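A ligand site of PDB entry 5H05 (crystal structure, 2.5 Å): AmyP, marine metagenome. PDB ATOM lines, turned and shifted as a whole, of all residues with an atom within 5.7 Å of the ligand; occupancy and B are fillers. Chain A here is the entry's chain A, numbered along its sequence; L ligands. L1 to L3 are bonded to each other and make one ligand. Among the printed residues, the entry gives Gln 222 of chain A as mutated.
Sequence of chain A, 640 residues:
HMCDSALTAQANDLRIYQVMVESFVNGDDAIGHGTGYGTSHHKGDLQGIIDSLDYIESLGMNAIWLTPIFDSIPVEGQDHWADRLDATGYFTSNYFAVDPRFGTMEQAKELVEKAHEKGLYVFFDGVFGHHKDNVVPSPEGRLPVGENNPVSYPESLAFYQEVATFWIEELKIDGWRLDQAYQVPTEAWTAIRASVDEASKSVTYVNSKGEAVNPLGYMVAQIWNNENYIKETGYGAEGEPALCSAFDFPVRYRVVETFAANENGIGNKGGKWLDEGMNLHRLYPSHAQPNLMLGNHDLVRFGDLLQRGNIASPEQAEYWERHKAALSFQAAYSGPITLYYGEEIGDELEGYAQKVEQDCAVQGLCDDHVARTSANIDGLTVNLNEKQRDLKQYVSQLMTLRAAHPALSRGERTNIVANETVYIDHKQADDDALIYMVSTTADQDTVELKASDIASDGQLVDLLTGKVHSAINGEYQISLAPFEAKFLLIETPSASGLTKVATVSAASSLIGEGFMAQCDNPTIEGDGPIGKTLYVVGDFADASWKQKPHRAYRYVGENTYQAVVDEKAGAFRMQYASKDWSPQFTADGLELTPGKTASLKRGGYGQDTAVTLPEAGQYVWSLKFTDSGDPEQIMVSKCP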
ATOM      1  N   MET A  20      -1.837 -34.550 -17.437  1.00  0.00           N
ATOM      2  CA  MET A  20      -2.175 -34.714 -16.025  1.00  0.00           C
ATOM      3  C   MET A  20      -2.755 -36.121 -15.846  1.00  0.00           C
ATOM      4  O   MET A  20      -3.856 -36.400 -16.334  1.00  0.00           O
ATOM      5  CB  MET A  20      -3.158 -33.638 -15.576  1.00  0.00           C
ATOM      6  CG  MET A  20      -3.675 -33.828 -14.162  1.00  0.00           C
ATOM      7  SD  MET A  20      -2.915 -32.680 -12.979  1.00  0.00           S
ATOM      8  CE  MET A  20      -3.135 -33.578 -11.434  1.00  0.00           C
ATOM      9  N   TYR A  37      -9.267 -33.657  -7.843  1.00  0.00           N
ATOM     10  CA  TYR A  37      -9.626 -32.253  -7.974  1.00  0.00           C
ATOM     11  C   TYR A  37      -9.840 -31.993  -9.453  1.00  0.00           C
ATOM     12  O   TYR A  37      -8.894 -32.105 -10.237  1.00  0.00           O
ATOM     13  CB  TYR A  37      -8.553 -31.344  -7.407  1.00  0.00           C
ATOM     14  CG  TYR A  37      -8.460 -31.239  -5.900  1.00  0.00           C
ATOM     15  CD1 TYR A  37      -9.475 -30.622  -5.156  1.00  0.00           C
ATOM     16  CD2 TYR A  37      -7.345 -31.691  -5.219  1.00  0.00           C
ATOM     17  CE1 TYR A  37      -9.360 -30.494  -3.755  1.00  0.00           C
ATOM     18  CE2 TYR A  37      -7.230 -31.570  -3.826  1.00  0.00           C
ATOM     19  CZ  TYR A  37      -8.244 -30.965  -3.098  1.00  0.00           C
ATOM     20  OH  TYR A  37      -8.113 -30.845  -1.729  1.00  0.00           O
ATOM     21  N   TRP A  81     -10.307 -34.559   1.472  1.00  0.00           N
ATOM     22  CA  TRP A  81      -9.358 -33.652   0.844  1.00  0.00           C
ATOM     23  C   TRP A  81      -8.023 -34.354   0.583  1.00  0.00           C
ATOM     24  O   TRP A  81      -7.445 -34.244  -0.512  1.00  0.00           O
ATOM     25  CB  TRP A  81      -9.148 -32.408   1.706  1.00  0.00           C
ATOM     26  CG  TRP A  81     -10.389 -31.652   2.093  1.00  0.00           C
ATOM     27  CD1 TRP A  81     -10.933 -31.536   3.356  1.00  0.00           C
ATOM     28  CD2 TRP A  81     -11.238 -30.885   1.226  1.00  0.00           C
ATOM     29  NE1 TRP A  81     -12.059 -30.736   3.306  1.00  0.00           N
ATOM     30  CE2 TRP A  81     -12.273 -30.334   2.020  1.00  0.00           C
ATOM     31  CE3 TRP A  81     -11.232 -30.611  -0.142  1.00  0.00           C
ATOM     32  CZ2 TRP A  81     -13.284 -29.538   1.494  1.00  0.00           C
ATOM     33  CZ3 TRP A  81     -12.244 -29.815  -0.669  1.00  0.00           C
ATOM     34  CH2 TRP A  81     -13.252 -29.288   0.145  1.00  0.00           C
ATOM     35  N   LEU A  85      -6.015 -34.927  -2.930  1.00  0.00           N
ATOM     36  CA  LEU A  85      -4.614 -34.545  -3.084  1.00  0.00           C
ATOM     37  C   LEU A  85      -3.775 -35.725  -3.545  1.00  0.00           C
ATOM     38  O   LEU A  85      -2.892 -35.566  -4.391  1.00  0.00           O
ATOM     39  CB  LEU A  85      -4.066 -34.017  -1.765  1.00  0.00           C
ATOM     40  CG  LEU A  85      -2.857 -33.105  -1.882  1.00  0.00           C
ATOM     41  CD1 LEU A  85      -3.182 -31.941  -2.814  1.00  0.00           C
ATOM     42  CD2 LEU A  85      -2.404 -32.559  -0.517  1.00  0.00           C
ATOM     43  N   THR A  88      -3.456 -36.116  -7.265  1.00  0.00           N
ATOM     44  CA  THR A  88      -2.693 -35.150  -8.047  1.00  0.00           C
ATOM     45  C   THR A  88      -1.225 -35.528  -8.176  1.00  0.00           C
ATOM     46  O   THR A  88      -0.572 -35.133  -9.150  1.00  0.00           O
ATOM     47  CB  THR A  88      -2.744 -33.755  -7.437  1.00  0.00           C
ATOM     48  OG1 THR A  88      -1.931 -33.744  -6.278  1.00  0.00           O
ATOM     49  CG2 THR A  88      -4.168 -33.346  -7.078  1.00  0.00           C
ATOM     50  N   TYR A  90       1.120 -34.389  -6.162  1.00  0.00           N
ATOM     51  CA  TYR A  90       1.973 -33.266  -5.807  1.00  0.00           C
ATOM     52  C   TYR A  90       2.411 -33.288  -4.342  1.00  0.00           C
ATOM     53  O   TYR A  90       3.251 -32.463  -3.957  1.00  0.00           O
ATOM     54  CB  TYR A  90       1.271 -31.955  -6.167  1.00  0.00           C
ATOM     55  CG  TYR A  90       1.489 -31.678  -7.633  1.00  0.00           C
ATOM     56  CD1 TYR A  90       2.758 -31.357  -8.099  1.00  0.00           C
ATOM     57  CD2 TYR A  90       0.457 -31.820  -8.570  1.00  0.00           C
ATOM     58  CE1 TYR A  90       3.002 -31.139  -9.442  1.00  0.00           C
ATOM     59  CE2 TYR A  90       0.701 -31.621  -9.937  1.00  0.00           C
ATOM     60  CZ  TYR A  90       1.984 -31.263 -10.354  1.00  0.00           C
ATOM     61  OH  TYR A  90       2.275 -31.034 -11.666  1.00  0.00           O
ATOM     62  N   PHE A  91       1.903 -34.230  -3.546  1.00  0.00           N
ATOM     63  CA  PHE A  91       2.270 -34.351  -2.145  1.00  0.00           C
ATOM     64  C   PHE A  91       2.482 -35.841  -1.876  1.00  0.00           C
ATOM     65  O   PHE A  91       1.630 -36.499  -1.287  1.00  0.00           O
ATOM     66  CB  PHE A  91       1.195 -33.759  -1.245  1.00  0.00           C
ATOM     67  CG  PHE A  91       1.245 -32.277  -1.170  1.00  0.00           C
ATOM     68  CD1 PHE A  91       0.726 -31.490  -2.194  1.00  0.00           C
ATOM     69  CD2 PHE A  91       1.840 -31.646  -0.083  1.00  0.00           C
ATOM     70  CE1 PHE A  91       0.793 -30.096  -2.126  1.00  0.00           C
ATOM     71  CE2 PHE A  91       1.921 -30.258   0.003  1.00  0.00           C
ATOM     72  CZ  PHE A  91       1.394 -29.483  -1.025  1.00  0.00           C
ATOM     73  N   VAL A 127       8.870 -32.869  -7.400  1.00  0.00           N
ATOM     74  CA  VAL A 127       8.467 -31.936  -6.352  1.00  0.00           C
ATOM     75  C   VAL A 127       9.522 -32.020  -5.263  1.00  0.00           C
ATOM     76  O   VAL A 127       9.452 -32.898  -4.402  1.00  0.00           O
ATOM     77  CB  VAL A 127       7.071 -32.253  -5.792  1.00  0.00           C
ATOM     78  CG1 VAL A 127       6.658 -31.192  -4.742  1.00  0.00           C
ATOM     79  CG2 VAL A 127       6.053 -32.346  -6.919  1.00  0.00           C
ATOM     80  N   HIS A 130       8.471 -29.962  -1.218  1.00  0.00           N
ATOM     81  CA  HIS A 130       7.457 -30.353  -0.246  1.00  0.00           C
ATOM     82  C   HIS A 130       7.013 -31.782  -0.552  1.00  0.00           C
ATOM     83  O   HIS A 130       7.327 -32.330  -1.612  1.00  0.00           O
ATOM     84  CB  HIS A 130       6.256 -29.385  -0.239  1.00  0.00           C
ATOM     85  CG  HIS A 130       5.550 -29.269  -1.558  1.00  0.00           C
ATOM     86  ND1 HIS A 130       5.755 -28.213  -2.427  1.00  0.00           N
ATOM     87  CD2 HIS A 130       4.633 -30.072  -2.165  1.00  0.00           C
ATOM     88  CE1 HIS A 130       4.994 -28.366  -3.498  1.00  0.00           C
ATOM     89  NE2 HIS A 130       4.308 -29.481  -3.360  1.00  0.00           N
ATOM     90  N   ARG A 177      10.450 -31.705 -14.873  1.00  0.00           N
ATOM     91  CA  ARG A 177       9.776 -30.454 -14.615  1.00  0.00           C
ATOM     92  C   ARG A 177       9.781 -30.235 -13.097  1.00  0.00           C
ATOM     93  O   ARG A 177       9.496 -31.160 -12.333  1.00  0.00           O
ATOM     94  CB  ARG A 177       8.365 -30.493 -15.199  1.00  0.00           C
ATOM     95  CG  ARG A 177       7.545 -29.262 -14.993  1.00  0.00           C
ATOM     96  CD  ARG A 177       6.668 -29.470 -13.817  1.00  0.00           C
ATOM     97  NE  ARG A 177       5.662 -28.432 -13.720  1.00  0.00           N
ATOM     98  CZ  ARG A 177       4.856 -28.308 -12.674  1.00  0.00           C
ATOM     99  NH1 ARG A 177       4.976 -29.152 -11.656  1.00  0.00           N
ATOM    100  NH2 ARG A 177       3.959 -27.341 -12.645  1.00  0.00           N
ATOM    101  N   ASP A 179       8.694 -28.606  -9.758  1.00  0.00           N
ATOM    102  CA  ASP A 179       7.501 -27.979  -9.219  1.00  0.00           C
ATOM    103  C   ASP A 179       7.841 -26.923  -8.180  1.00  0.00           C
ATOM    104  O   ASP A 179       8.738 -27.111  -7.358  1.00  0.00           O
ATOM    105  CB  ASP A 179       6.609 -29.028  -8.592  1.00  0.00           C
ATOM    106  CG  ASP A 179       5.332 -28.433  -8.081  1.00  0.00           C
ATOM    107  OD1 ASP A 179       4.667 -27.794  -8.919  1.00  0.00           O
ATOM    108  OD2 ASP A 179       5.031 -28.550  -6.870  1.00  0.00           O
ATOM    109  N   GLN A 180       7.065 -25.819  -8.190  1.00  0.00           N
ATOM    110  CA  GLN A 180       7.285 -24.661  -7.324  1.00  0.00           C
ATOM    111  C   GLN A 180       8.758 -24.406  -7.020  1.00  0.00           C
ATOM    112  O   GLN A 180       9.155 -24.325  -5.853  1.00  0.00           O
ATOM    113  CB  GLN A 180       6.501 -24.799  -6.022  1.00  0.00           C
ATOM    114  CG  GLN A 180       5.066 -24.442  -6.193  1.00  0.00           C
ATOM    115  CD  GLN A 180       4.254 -24.680  -4.954  1.00  0.00           C
ATOM    116  OE1 GLN A 180       4.650 -25.439  -4.082  1.00  0.00           O
ATOM    117  NE2 GLN A 180       3.106 -24.035  -4.871  1.00  0.00           N
ATOM    118  N   GLN A 222       9.103 -24.621 -12.820  1.00  0.00           N
ATOM    119  CA  GLN A 222       7.831 -23.932 -12.763  1.00  0.00           C
ATOM    120  C   GLN A 222       7.890 -22.872 -11.672  1.00  0.00           C
ATOM    121  O   GLN A 222       7.965 -23.186 -10.485  1.00  0.00           O
ATOM    122  CB  GLN A 222       6.676 -24.882 -12.514  1.00  0.00           C
ATOM    123  CG  GLN A 222       5.384 -24.225 -12.953  1.00  0.00           C
ATOM    124  CD  GLN A 222       4.404 -24.258 -11.840  1.00  0.00           C
ATOM    125  OE1 GLN A 222       4.734 -24.691 -10.730  1.00  0.00           O
ATOM    126  NE2 GLN A 222       3.177 -23.811 -12.101  1.00  0.00           N
ATOM    127  N   TRP A 224       5.582 -19.570 -11.011  1.00  0.00           N
ATOM    128  CA  TRP A 224       4.382 -18.846 -11.410  1.00  0.00           C
ATOM    129  C   TRP A 224       4.475 -17.394 -10.930  1.00  0.00           C
ATOM    130  O   TRP A 224       3.855 -16.998  -9.951  1.00  0.00           O
ATOM    131  CB  TRP A 224       3.155 -19.548 -10.862  1.00  0.00           C
ATOM    132  CG  TRP A 224       1.870 -19.142 -11.473  1.00  0.00           C
ATOM    133  CD1 TRP A 224       1.647 -18.070 -12.279  1.00  0.00           C
ATOM    134  CD2 TRP A 224       0.621 -19.803 -11.325  1.00  0.00           C
ATOM    135  NE1 TRP A 224       0.325 -18.016 -12.641  1.00  0.00           N
ATOM    136  CE2 TRP A 224      -0.330 -19.083 -12.069  1.00  0.00           C
ATOM    137  CE3 TRP A 224       0.203 -20.945 -10.624  1.00  0.00           C
ATOM    138  CZ2 TRP A 224      -1.674 -19.443 -12.135  1.00  0.00           C
ATOM    139  CZ3 TRP A 224      -1.121 -21.311 -10.684  1.00  0.00           C
ATOM    140  CH2 TRP A 224      -2.056 -20.563 -11.437  1.00  0.00           C
ATOM    141  N   HIS A 297      -2.359 -27.669 -16.113  1.00  0.00           N
ATOM    142  CA  HIS A 297      -3.347 -28.191 -15.191  1.00  0.00           C
ATOM    143  C   HIS A 297      -3.744 -27.192 -14.092  1.00  0.00           C
ATOM    144  O   HIS A 297      -4.637 -27.510 -13.301  1.00  0.00           O
ATOM    145  CB  HIS A 297      -2.787 -29.466 -14.571  1.00  0.00           C
ATOM    146  CG  HIS A 297      -1.605 -29.207 -13.696  1.00  0.00           C
ATOM    147  ND1 HIS A 297      -0.393 -28.792 -14.198  1.00  0.00           N
ATOM    148  CD2 HIS A 297      -1.464 -29.210 -12.344  1.00  0.00           C
ATOM    149  CE1 HIS A 297       0.460 -28.600 -13.205  1.00  0.00           C
ATOM    150  NE2 HIS A 297      -0.175 -28.844 -12.069  1.00  0.00           N
ATOM    151  N   ASP A 298      -3.112 -26.018 -13.999  1.00  0.00           N
ATOM    152  CA  ASP A 298      -3.447 -25.003 -12.988  1.00  0.00           C
ATOM    153  C   ASP A 298      -4.161 -23.812 -13.584  1.00  0.00           C
ATOM    154  O   ASP A 298      -4.546 -22.906 -12.845  1.00  0.00           O
ATOM    155  CB  ASP A 298      -2.187 -24.483 -12.276  1.00  0.00           C
ATOM    156  CG  ASP A 298      -1.427 -25.572 -11.554  1.00  0.00           C
ATOM    157  OD1 ASP A 298      -2.078 -26.515 -11.066  1.00  0.00           O
ATOM    158  OD2 ASP A 298      -0.164 -25.480 -11.497  1.00  0.00           O
ATOM    159  N   CYS A 360     -15.998 -24.392  -4.551  1.00  0.00           N
ATOM    160  CA  CYS A 360     -15.617 -24.795  -5.901  1.00  0.00           C
ATOM    161  C   CYS A 360     -14.826 -26.098  -5.924  1.00  0.00           C
ATOM    162  O   CYS A 360     -14.981 -26.869  -6.888  1.00  0.00           O
ATOM    163  CB  CYS A 360     -14.823 -23.677  -6.622  1.00  0.00           C
ATOM    164  SG  CYS A 360     -13.217 -23.093  -5.949  1.00  0.00           S
ATOM    165  N   ALA A 361     -14.001 -26.366  -4.915  1.00  0.00           N
ATOM    166  CA  ALA A 361     -13.169 -27.568  -4.953  1.00  0.00           C
ATOM    167  C   ALA A 361     -14.021 -28.832  -5.084  1.00  0.00           C
ATOM    168  O   ALA A 361     -13.753 -29.670  -5.957  1.00  0.00           O
ATOM    169  CB  ALA A 361     -12.279 -27.643  -3.711  1.00  0.00           C
ATOM    170  N   CYS A 366     -12.670 -24.874  -9.364  1.00  0.00           N
ATOM    171  CA  CYS A 366     -11.781 -23.746  -9.114  1.00  0.00           C
ATOM    172  C   CYS A 366     -10.913 -23.504 -10.341  1.00  0.00           C
ATOM    173  O   CYS A 366     -10.605 -24.432 -11.105  1.00  0.00           O
ATOM    174  CB  CYS A 366     -10.897 -23.984  -7.897  1.00  0.00           C
ATOM    175  SG  CYS A 366     -11.794 -24.512  -6.396  1.00  0.00           S
ATOM    176  N   ASP A 368      -7.869 -23.125 -10.467  1.00  0.00           N
ATOM    177  CA  ASP A 368      -6.564 -23.777 -10.438  1.00  0.00           C
ATOM    178  C   ASP A 368      -6.629 -25.269 -10.734  1.00  0.00           C
ATOM    179  O   ASP A 368      -5.578 -25.929 -10.744  1.00  0.00           O
ATOM    180  CB  ASP A 368      -5.875 -23.544  -9.088  1.00  0.00           C
ATOM    181  CG  ASP A 368      -6.441 -24.412  -7.996  1.00  0.00           C
ATOM    182  OD1 ASP A 368      -7.679 -24.359  -7.784  1.00  0.00           O
ATOM    183  OD2 ASP A 368      -5.662 -25.176  -7.362  1.00  0.00           O
ATOM    184  N   HIS A 369      -7.815 -25.839 -10.960  1.00  0.00           N
ATOM    185  CA  HIS A 369      -7.869 -27.244 -11.375  1.00  0.00           C
ATOM    186  C   HIS A 369      -9.027 -27.548 -12.316  1.00  0.00           C
ATOM    187  O   HIS A 369      -9.255 -28.714 -12.618  1.00  0.00           O
ATOM    188  CB  HIS A 369      -7.943 -28.163 -10.139  1.00  0.00           C
ATOM    189  CG  HIS A 369      -9.170 -27.967  -9.327  1.00  0.00           C
ATOM    190  ND1 HIS A 369      -9.148 -27.505  -8.038  1.00  0.00           N
ATOM    191  CD2 HIS A 369     -10.484 -28.137  -9.642  1.00  0.00           C
ATOM    192  CE1 HIS A 369     -10.386 -27.417  -7.574  1.00  0.00           C
ATOM    193  NE2 HIS A 369     -11.207 -27.794  -8.523  1.00  0.00           N
ATOM    194  N   ARG A 372      -8.585 -29.836 -15.516  1.00  0.00           N
ATOM    195  CA  ARG A 372      -8.307 -31.252 -15.353  1.00  0.00           C
ATOM    196  C   ARG A 372      -9.579 -32.045 -15.712  1.00  0.00           C
ATOM    197  O   ARG A 372     -10.212 -32.721 -14.900  1.00  0.00           O
ATOM    198  CB  ARG A 372      -7.833 -31.522 -13.947  1.00  0.00           C
ATOM    199  CG  ARG A 372      -6.657 -30.644 -13.581  1.00  0.00           C
ATOM    200  CD  ARG A 372      -6.162 -30.920 -12.170  1.00  0.00           C
ATOM    201  NE  ARG A 372      -5.358 -29.795 -11.704  1.00  0.00           N
ATOM    202  CZ  ARG A 372      -4.814 -29.706 -10.499  1.00  0.00           C
ATOM    203  NH1 ARG A 372      -4.110 -28.635 -10.172  1.00  0.00           N
ATOM    204  NH2 ARG A 372      -4.981 -30.677  -9.619  1.00  0.00           N
HETATM  205  C1  LIG L   1       2.417 -26.334  -8.149  1.00  0.00           C
HETATM  206  C2  LIG L   1       1.560 -27.338  -8.939  1.00  0.00           C
HETATM  207  C3  LIG L   1       0.207 -27.383  -8.312  1.00  0.00           C
HETATM  208  C4  LIG L   1       0.324 -27.850  -6.890  1.00  0.00           C
HETATM  209  C5  LIG L   1       1.163 -26.866  -6.058  1.00  0.00           C
HETATM  210  C6  LIG L   1       2.258 -27.510  -5.293  1.00  0.00           C
HETATM  211  O1  LIG L   1       2.835 -25.258  -8.887  1.00  0.00           O
HETATM  212  O2  LIG L   1       1.456 -27.057 -10.355  1.00  0.00           O
HETATM  213  O3  LIG L   1      -0.670 -28.226  -9.128  1.00  0.00           O
HETATM  214  O4  LIG L   1      -0.973 -27.909  -6.275  1.00  0.00           O
HETATM  215  O5  LIG L   1       1.757 -25.820  -6.908  1.00  0.00           O
HETATM  216  O6  LIG L   1       2.444 -28.823  -5.734  1.00  0.00           O
HETATM  217  C1  LG2 L   2      -1.209 -29.157  -5.828  1.00  0.00           C
HETATM  218  C2  LG2 L   2      -2.437 -29.724  -6.515  1.00  0.00           C
HETATM  219  C3  LG2 L   2      -3.581 -28.814  -6.322  1.00  0.00           C
HETATM  220  C4  LG2 L   2      -3.824 -28.649  -4.846  1.00  0.00           C
HETATM  221  C5  LG2 L   2      -2.576 -28.046  -4.225  1.00  0.00           C
HETATM  222  C6  LG2 L   2      -2.778 -27.774  -2.781  1.00  0.00           C
HETATM  223  O1  LG2 L   2      -2.164 -29.915  -7.918  1.00  0.00           O
HETATM  224  O2  LG2 L   2      -4.748 -29.387  -6.976  1.00  0.00           O
HETATM  225  O3  LG2 L   2      -4.897 -27.732  -4.555  1.00  0.00           O
HETATM  226  O4  LG2 L   2      -1.479 -28.992  -4.378  1.00  0.00           O
HETATM  227  O5  LG2 L   2      -1.540 -27.467  -2.195  1.00  0.00           O
HETATM  228  C1  LG3 L   3      -6.094 -28.403  -4.449  1.00  0.00           C
HETATM  229  C2  LG3 L   3      -7.163 -27.656  -5.230  1.00  0.00           C
HETATM  230  C3  LG3 L   3      -7.348 -26.286  -4.657  1.00  0.00           C
HETATM  231  C4  LG3 L   3      -7.649 -26.350  -3.194  1.00  0.00           C
HETATM  232  C5  LG3 L   3      -6.596 -27.137  -2.420  1.00  0.00           C
HETATM  233  C6  LG3 L   3      -6.990 -27.263  -0.988  1.00  0.00           C
HETATM  234  O1  LG3 L   3      -6.744 -27.576  -6.625  1.00  0.00           O
HETATM  235  O2  LG3 L   3      -8.401 -25.547  -5.343  1.00  0.00           O
HETATM  236  O3  LG3 L   3      -7.634 -25.020  -2.671  1.00  0.00           O
HETATM  237  O4  LG3 L   3      -6.445 -28.477  -2.993  1.00  0.00           O
HETATM  238  O5  LG3 L   3      -8.169 -28.017  -0.906  1.00  0.00           O
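Merely in contact with the ligand: Leu 85 (3.7 Å), Thr 88 (3.9 Å), Tyr 90 (3.3 Å) and Phe 91 (3.4 Å). 16 residues have an atom within 4 Å of the ligand: Tyr 37, Leu 85, Thr 88, Tyr 90, Phe 91, His 130, Arg 177, Asp 179, Gln 180, Gln 222, His 297, Asp 298, Cys 366, Asp 368, His 369 and Arg 372.
The side-chain amide oxygen (OE1) of Gln 222 sits at hydrogen-bond distance from an oxygen (O1) of LIG L1, 2.7 Å away. A ring nitrogen (NE2) of His 130 is in hydrogen-bond range of an oxygen (O6) of LIG L1 (3.1 Å). The guanidinium group (NH2) of Arg 372 sits at hydrogen-bond distance from an oxygen (O2) of LG2 L2, 3.0 Å away. The side-chain carboxylate of Asp 368 is in hydrogen-bond range of an oxygen (O1) of LG3 L3, at 2.7 Å. An oxygen (O2) of LIG L1 sits at hydrogen-bond distance from the guanidinium group (NH2) of Arg 177 (3.4 Å). O2 of LIG L1 is in hydrogen-bond range of OD2 of Asp 298 (2.5 Å). The side-chain sulfur of Cys 366 sits at hydrogen-bond distance from an oxygen (O2) of LG3 L3, 3.7 Å away. OD2 of Asp 179 sits at hydrogen-bond distance from O6 of LIG L1 (2.8 Å). ND1 of His 369 sits at hydrogen-bond distance from O1 of LG3 L3, 2.8 Å away. An oxygen (O5) of LIG L1 sits at hydrogen-bond distance from the side-chain amide nitrogen (NE2) of Gln 180, at 3.0 Å. The side-chain hydroxyl of Tyr 37 is in hydrogen-bond range of an oxygen (O5) of LG3 L3 (2.9 Å). An oxygen (O2) of LIG L1 is in hydrogen-bond range of a ring nitrogen (NE2) of His 297 (3.0 Å).
A ring nitrogen (ND1) of His 130 lies close to the side-chain amide oxygen (OE1) of Gln 180, 3.4 Å away. OD1 of Asp 179 is in salt-bridge range of NH1 of Arg 177. OG1 of Thr 88 sits at hydrogen-bond distance from N of Tyr 90 (3.1 Å). The backbone carbonyl oxygen of Leu 85 sits at hydrogen-bond distance from the side-chain hydroxyl of Thr 88 (2.8 Å). O of His 297 sits at hydrogen-bond distance from NE of Arg 372 (2.9 Å). SG of Cys 366 is in hydrogen-bond range of N of Ala 361 (3.2 Å). NE2 of His 297 lies close to OD1 of Asp 298, 3.2 Å away. NH1 of Arg 372 lies within salt-bridge range of OD1 of Asp 298, at 3.1 Å.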
